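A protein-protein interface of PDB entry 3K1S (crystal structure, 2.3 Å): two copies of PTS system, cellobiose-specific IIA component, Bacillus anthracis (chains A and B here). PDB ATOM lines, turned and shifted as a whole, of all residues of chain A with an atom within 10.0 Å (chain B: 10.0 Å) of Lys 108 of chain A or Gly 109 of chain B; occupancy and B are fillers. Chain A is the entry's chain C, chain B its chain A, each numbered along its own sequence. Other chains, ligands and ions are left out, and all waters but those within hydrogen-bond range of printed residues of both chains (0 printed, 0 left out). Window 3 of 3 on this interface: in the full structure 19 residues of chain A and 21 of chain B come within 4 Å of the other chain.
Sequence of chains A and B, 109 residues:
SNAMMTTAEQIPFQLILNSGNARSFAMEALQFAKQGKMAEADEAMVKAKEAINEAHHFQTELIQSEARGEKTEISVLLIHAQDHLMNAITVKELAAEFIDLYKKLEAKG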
ATOM      1  N   ASP A 100      -1.624  -2.533  21.643  1.00  0.00           N
ATOM      2  CA  ASP A 100      -1.714  -1.163  22.146  1.00  0.00           C
ATOM      3  C   ASP A 100      -3.003  -0.464  21.724  1.00  0.00           C
ATOM      4  O   ASP A 100      -3.645   0.199  22.542  1.00  0.00           O
ATOM      5  CB  ASP A 100      -0.505  -0.333  21.706  1.00  0.00           C
ATOM      6  CG  ASP A 100       0.704  -0.548  22.593  1.00  0.00           C
ATOM      7  OD1 ASP A 100       0.522  -0.914  23.774  1.00  0.00           O
ATOM      8  OD2 ASP A 100       1.841  -0.342  22.111  1.00  0.00           O
ATOM      9  N   LEU A 101      -3.374  -0.607  20.451  1.00  0.00           N
ATOM     10  CA  LEU A 101      -4.628  -0.039  19.947  1.00  0.00           C
ATOM     11  C   LEU A 101      -5.831  -0.563  20.728  1.00  0.00           C
ATOM     12  O   LEU A 101      -6.722   0.209  21.105  1.00  0.00           O
ATOM     13  CB  LEU A 101      -4.809  -0.308  18.448  1.00  0.00           C
ATOM     14  CG  LEU A 101      -4.301   0.736  17.445  1.00  0.00           C
ATOM     15  CD1 LEU A 101      -4.279   0.157  16.044  1.00  0.00           C
ATOM     16  CD2 LEU A 101      -5.150   1.997  17.481  1.00  0.00           C
ATOM     17  N   TYR A 102      -5.853  -1.870  20.976  1.00  0.00           N
ATOM     18  CA  TYR A 102      -6.959  -2.469  21.716  1.00  0.00           C
ATOM     19  C   TYR A 102      -6.993  -1.997  23.169  1.00  0.00           C
ATOM     20  O   TYR A 102      -8.052  -1.629  23.672  1.00  0.00           O
ATOM     21  CB  TYR A 102      -6.961  -3.997  21.597  1.00  0.00           C
ATOM     22  CG  TYR A 102      -7.486  -4.480  20.261  1.00  0.00           C
ATOM     23  CD1 TYR A 102      -8.837  -4.338  19.931  1.00  0.00           C
ATOM     24  CD2 TYR A 102      -6.633  -5.065  19.318  1.00  0.00           C
ATOM     25  CE1 TYR A 102      -9.329  -4.770  18.707  1.00  0.00           C
ATOM     26  CE2 TYR A 102      -7.119  -5.502  18.079  1.00  0.00           C
ATOM     27  CZ  TYR A 102      -8.469  -5.350  17.786  1.00  0.00           C
ATOM     28  OH  TYR A 102      -8.970  -5.776  16.578  1.00  0.00           O
ATOM     29  N   LYS A 103      -5.833  -1.977  23.825  1.00  0.00           N
ATOM     30  CA  LYS A 103      -5.733  -1.427  25.182  1.00  0.00           C
ATOM     31  C   LYS A 103      -6.203   0.027  25.219  1.00  0.00           C
ATOM     32  O   LYS A 103      -6.879   0.443  26.162  1.00  0.00           O
ATOM     33  CB  LYS A 103      -4.305  -1.547  25.736  1.00  0.00           C
ATOM     34  CG  LYS A 103      -3.863  -2.981  26.011  1.00  0.00           C
ATOM     35  CD  LYS A 103      -2.450  -3.048  26.586  1.00  0.00           C
ATOM     36  CE  LYS A 103      -2.054  -4.483  26.890  1.00  0.00           C
ATOM     37  NZ  LYS A 103      -0.612  -4.611  27.237  1.00  0.00           N
ATOM     38  N   LYS A 104      -5.848   0.790  24.187  1.00  0.00           N
ATOM     39  CA  LYS A 104      -6.281   2.179  24.065  1.00  0.00           C
ATOM     40  C   LYS A 104      -7.811   2.278  24.066  1.00  0.00           C
ATOM     41  O   LYS A 104      -8.394   3.012  24.870  1.00  0.00           O
ATOM     42  CB  LYS A 104      -5.700   2.817  22.798  1.00  0.00           C
ATOM     43  CG  LYS A 104      -5.993   4.302  22.678  1.00  0.00           C
ATOM     44  CD  LYS A 104      -5.597   4.856  21.322  1.00  0.00           C
ATOM     45  CE  LYS A 104      -5.929   6.342  21.227  1.00  0.00           C
ATOM     46  NZ  LYS A 104      -5.090   7.171  22.145  1.00  0.00           N
ATOM     47  N   LEU A 105      -8.449   1.522  23.173  1.00  0.00           N
ATOM     48  CA  LEU A 105      -9.906   1.512  23.045  1.00  0.00           C
ATOM     49  C   LEU A 105     -10.620   1.103  24.335  1.00  0.00           C
ATOM     50  O   LEU A 105     -11.685   1.640  24.653  1.00  0.00           O
ATOM     51  CB  LEU A 105     -10.336   0.613  21.882  1.00  0.00           C
ATOM     52  CG  LEU A 105      -9.944   1.085  20.483  1.00  0.00           C
ATOM     53  CD1 LEU A 105     -10.047  -0.058  19.494  1.00  0.00           C
ATOM     54  CD2 LEU A 105     -10.802   2.267  20.041  1.00  0.00           C
ATOM     55  N   GLU A 106     -10.034   0.158  25.067  1.00  0.00           N
ATOM     56  CA  GLU A 106     -10.544  -0.229  26.384  1.00  0.00           C
ATOM     57  C   GLU A 106     -10.547   0.955  27.353  1.00  0.00           C
ATOM     58  O   GLU A 106     -11.582   1.290  27.938  1.00  0.00           O
ATOM     59  CB  GLU A 106      -9.716  -1.375  26.976  1.00  0.00           C
ATOM     60  CG  GLU A 106     -10.160  -2.770  26.558  1.00  0.00           C
ATOM     61  CD  GLU A 106      -9.509  -3.873  27.386  1.00  0.00           C
ATOM     62  OE1 GLU A 106      -9.354  -3.701  28.617  1.00  0.00           O
ATOM     63  OE2 GLU A 106      -9.159  -4.921  26.804  1.00  0.00           O
ATOM     64  N   ALA A 107      -9.382   1.585  27.506  1.00  0.00           N
ATOM     65  CA  ALA A 107      -9.172   2.657  28.478  1.00  0.00           C
ATOM     66  C   ALA A 107     -10.166   3.814  28.336  1.00  0.00           C
ATOM     67  O   ALA A 107     -10.647   4.346  29.341  1.00  0.00           O
ATOM     68  CB  ALA A 107      -7.737   3.170  28.400  1.00  0.00           C
ATOM     69  N   LYS A 108     -10.464   4.197  27.096  1.00  0.00           N
ATOM     70  CA  LYS A 108     -11.387   5.303  26.829  1.00  0.00           C
ATOM     71  C   LYS A 108     -12.844   4.938  27.139  1.00  0.00           C
ATOM     72  O   LYS A 108     -13.727   5.803  27.124  1.00  0.00           O
ATOM     73  CB  LYS A 108     -11.234   5.820  25.390  1.00  0.00           C
ATOM     74  CG  LYS A 108     -11.818   4.921  24.299  1.00  0.00           C
ATOM     75  CD  LYS A 108     -11.843   5.625  22.939  1.00  0.00           C
ATOM     76  CE  LYS A 108     -12.953   6.675  22.854  1.00  0.00           C
ATOM     77  NZ  LYS A 108     -12.948   7.409  21.554  1.00  0.00           N
ATOM     78  N   GLY A 109     -13.080   3.658  27.422  1.00  0.00           N
ATOM     79  CA  GLY A 109     -14.416   3.149  27.721  1.00  0.00           C
ATOM     80  C   GLY A 109     -14.524   1.657  27.465  1.00  0.00           C
ATOM     81  O   GLY A 109     -14.080   1.159  26.426  1.00  0.00           O
ATOM     82  OXT GLY A 109     -15.058   0.911  28.290  1.00  0.00           O
ATOM     83  N   LEU B 101      -5.408   5.024  10.987  1.00  0.00           N
ATOM     84  CA  LEU B 101      -6.254   4.529  12.059  1.00  0.00           C
ATOM     85  C   LEU B 101      -6.176   5.434  13.289  1.00  0.00           C
ATOM     86  O   LEU B 101      -7.186   5.670  13.952  1.00  0.00           O
ATOM     87  CB  LEU B 101      -5.896   3.074  12.401  1.00  0.00           C
ATOM     88  CG  LEU B 101      -6.688   2.338  13.486  1.00  0.00           C
ATOM     89  CD1 LEU B 101      -8.193   2.446  13.273  1.00  0.00           C
ATOM     90  CD2 LEU B 101      -6.262   0.877  13.531  1.00  0.00           C
ATOM     91  N   TYR B 102      -4.989   5.949  13.589  1.00  0.00           N
ATOM     92  CA  TYR B 102      -4.850   6.911  14.691  1.00  0.00           C
ATOM     93  C   TYR B 102      -5.528   8.248  14.407  1.00  0.00           C
ATOM     94  O   TYR B 102      -6.057   8.880  15.325  1.00  0.00           O
ATOM     95  CB  TYR B 102      -3.385   7.111  15.094  1.00  0.00           C
ATOM     96  CG  TYR B 102      -2.884   6.039  16.034  1.00  0.00           C
ATOM     97  CD1 TYR B 102      -3.330   5.984  17.352  1.00  0.00           C
ATOM     98  CD2 TYR B 102      -1.970   5.074  15.605  1.00  0.00           C
ATOM     99  CE1 TYR B 102      -2.882   4.999  18.223  1.00  0.00           C
ATOM    100  CE2 TYR B 102      -1.515   4.080  16.473  1.00  0.00           C
ATOM    101  CZ  TYR B 102      -1.980   4.051  17.779  1.00  0.00           C
ATOM    102  OH  TYR B 102      -1.544   3.083  18.655  1.00  0.00           O
ATOM    103  N   LYS B 103      -5.517   8.671  13.143  1.00  0.00           N
ATOM    104  CA  LYS B 103      -6.232   9.886  12.732  1.00  0.00           C
ATOM    105  C   LYS B 103      -7.741   9.728  12.886  1.00  0.00           C
ATOM    106  O   LYS B 103      -8.423  10.664  13.312  1.00  0.00           O
ATOM    107  CB  LYS B 103      -5.874  10.301  11.303  1.00  0.00           C
ATOM    108  CG  LYS B 103      -4.521  10.992  11.200  1.00  0.00           C
ATOM    109  CD  LYS B 103      -4.105  11.241   9.762  1.00  0.00           C
ATOM    110  CE  LYS B 103      -2.721  11.873   9.725  1.00  0.00           C
ATOM    111  NZ  LYS B 103      -2.065  11.767   8.394  1.00  0.00           N
ATOM    112  N   LYS B 104      -8.253   8.544  12.553  1.00  0.00           N
ATOM    113  CA  LYS B 104      -9.683   8.256  12.687  1.00  0.00           C
ATOM    114  C   LYS B 104     -10.108   8.258  14.152  1.00  0.00           C
ATOM    115  O   LYS B 104     -11.173   8.771  14.495  1.00  0.00           O
ATOM    116  CB  LYS B 104     -10.046   6.913  12.043  1.00  0.00           C
ATOM    117  CG  LYS B 104     -11.544   6.738  11.813  1.00  0.00           C
ATOM    118  CD  LYS B 104     -11.961   5.273  11.787  1.00  0.00           C
ATOM    119  CE  LYS B 104     -13.300   5.078  11.073  1.00  0.00           C
ATOM    120  NZ  LYS B 104     -14.386   5.981  11.570  1.00  0.00           N
ATOM    121  N   LEU B 105      -9.267   7.680  15.009  1.00  0.00           N
ATOM    122  CA  LEU B 105      -9.557   7.602  16.438  1.00  0.00           C
ATOM    123  C   LEU B 105      -9.568   8.977  17.111  1.00  0.00           C
ATOM    124  O   LEU B 105     -10.272   9.178  18.100  1.00  0.00           O
ATOM    125  CB  LEU B 105      -8.583   6.654  17.137  1.00  0.00           C
ATOM    126  CG  LEU B 105      -8.612   5.189  16.687  1.00  0.00           C
ATOM    127  CD1 LEU B 105      -7.530   4.389  17.393  1.00  0.00           C
ATOM    128  CD2 LEU B 105      -9.982   4.553  16.915  1.00  0.00           C
ATOM    129  N   GLU B 106      -8.760   9.892  16.605  1.00  0.00           N
ATOM    130  CA  GLU B 106      -8.802  11.281  16.998  1.00  0.00           C
ATOM    131  C   GLU B 106     -10.058  11.981  16.515  1.00  0.00           C
ATOM    132  O   GLU B 106     -10.635  12.792  17.208  1.00  0.00           O
ATOM    133  CB  GLU B 106      -7.577  12.025  16.504  1.00  0.00           C
ATOM    134  CG  GLU B 106      -6.337  11.655  17.236  1.00  0.00           C
ATOM    135  CD  GLU B 106      -5.455  12.833  17.491  1.00  0.00           C
ATOM    136  OE1 GLU B 106      -5.488  13.783  16.687  1.00  0.00           O
ATOM    137  OE2 GLU B 106      -4.730  12.813  18.501  1.00  0.00           O
ATOM    138  N   ALA B 107     -10.457  11.664  15.298  1.00  0.00           N
ATOM    139  CA  ALA B 107     -11.621  12.268  14.657  1.00  0.00           C
ATOM    140  C   ALA B 107     -12.911  11.976  15.425  1.00  0.00           C
ATOM    141  O   ALA B 107     -13.875  12.741  15.342  1.00  0.00           O
ATOM    142  CB  ALA B 107     -11.736  11.789  13.217  1.00  0.00           C
ATOM    143  N   LYS B 108     -12.919  10.872  16.174  1.00  0.00           N
ATOM    144  CA  LYS B 108     -14.105  10.438  16.914  1.00  0.00           C
ATOM    145  C   LYS B 108     -14.161  11.034  18.328  1.00  0.00           C
ATOM    146  O   LYS B 108     -15.038  11.851  18.624  1.00  0.00           O
ATOM    147  CB  LYS B 108     -14.184   8.905  16.958  1.00  0.00           C
ATOM    148  CG  LYS B 108     -15.516   8.357  17.473  1.00  0.00           C
ATOM    149  CD  LYS B 108     -15.407   6.896  17.906  1.00  0.00           C
ATOM    150  CE  LYS B 108     -15.338   5.944  16.716  1.00  0.00           C
ATOM    151  NZ  LYS B 108     -15.212   4.526  17.151  1.00  0.00           N
ATOM    152  N   GLY B 109     -13.213  10.639  19.176  1.00  0.00           N
ATOM    153  CA  GLY B 109     -13.129  11.138  20.548  1.00  0.00           C
ATOM    154  C   GLY B 109     -12.590  12.555  20.625  1.00  0.00           C
ATOM    155  O   GLY B 109     -11.580  12.812  21.283  1.00  0.00           O
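Among the printed residues, merely in contact across the chains: Leu 101 of chain A with Leu 101 of chain B (3.3 Å), Leu 101 of chain A with Leu 105 of chain B (3.4 Å), Leu 101 of chain A with Tyr 102 of chain B (3.8 Å), Lys 108 of chain A with Gly 109 of chain B (3.9 Å) and Leu 105 of chain A with Leu 105 of chain B (3.96 Å).
Printed residues of chain B within 4 Å of Leu 101 of chain A: Leu 101 (3.3 Å), Tyr 102 (3.8 Å) and Leu 105 (3.4 Å).
Of the printed residues of chain B, Leu 105 of chain A touches Leu 105 (3.96 Å).
No residue of chain B comes within 4 Å of Ala 107 of chain A.
Gly 109 of chain A touches none of the printed residues of chain B.
Of the printed residues of chain A, Leu 101 of chain B touches Leu 101.
Printed residues of chain A within 4 Å of Tyr 102 of chain B: Leu 101 (3.8 Å).
Of the printed residues of chain A, Leu 105 of chain B touches Leu 101 (3.4 Å) and Leu 105 (3.96 Å).
No residue of chain A comes within 4 Å of Lys 108 of chain B.
Of the printed residues of chain A, Gly 109 of chain B touches Lys 108 (3.9 Å).
The nearest printed residue of chain B that does not touch Lys 108 of chain A is Lys 108 of chain B (4.4 Å).
The nearest printed residue of chain A that does not touch Leu 101 of chain B is Leu 105 of chain A (7.0 Å).
Of the 9 printed residues of chain B, 4 touch a printed residue of chain A.
Printed residues of chain B that touch a printed residue of chain A: Leu 101, Tyr 102, Leu 105 and Gly 109.
Hydrophobic or aromatic side chains of chain B that line the printed part of chain A: Leu 101, Tyr 102 and Leu 105.
Among the printed residues, no Asp or Glu carboxylate lies within 4 Å of a Lys or Arg side-chain nitrogen of the other chain.
Leu 101 of chain A touches Tyr 102 of chain B, but with the chains exchanged Tyr 102 of chain A does not touch Leu 101 of chain B (7.8 Å).
Leu 101 of chain A touches Leu 105 of chain B, but with the chains exchanged Leu 105 of chain A does not touch Leu 101 of chain B (7.0 Å).
Leu 105 of chain B touches its own counterpart, Leu 105 of chain A.
Lys 108 of chain A touches Gly 109 of chain B, but with the chains exchanged Gly 109 of chain A does not touch Lys 108 of chain B (9.9 Å).
9 positions are printed for both chains.
Of the 5 pairs that touch across the chains among the printed residues, 2 have their exchanged pair printed and touching as well.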
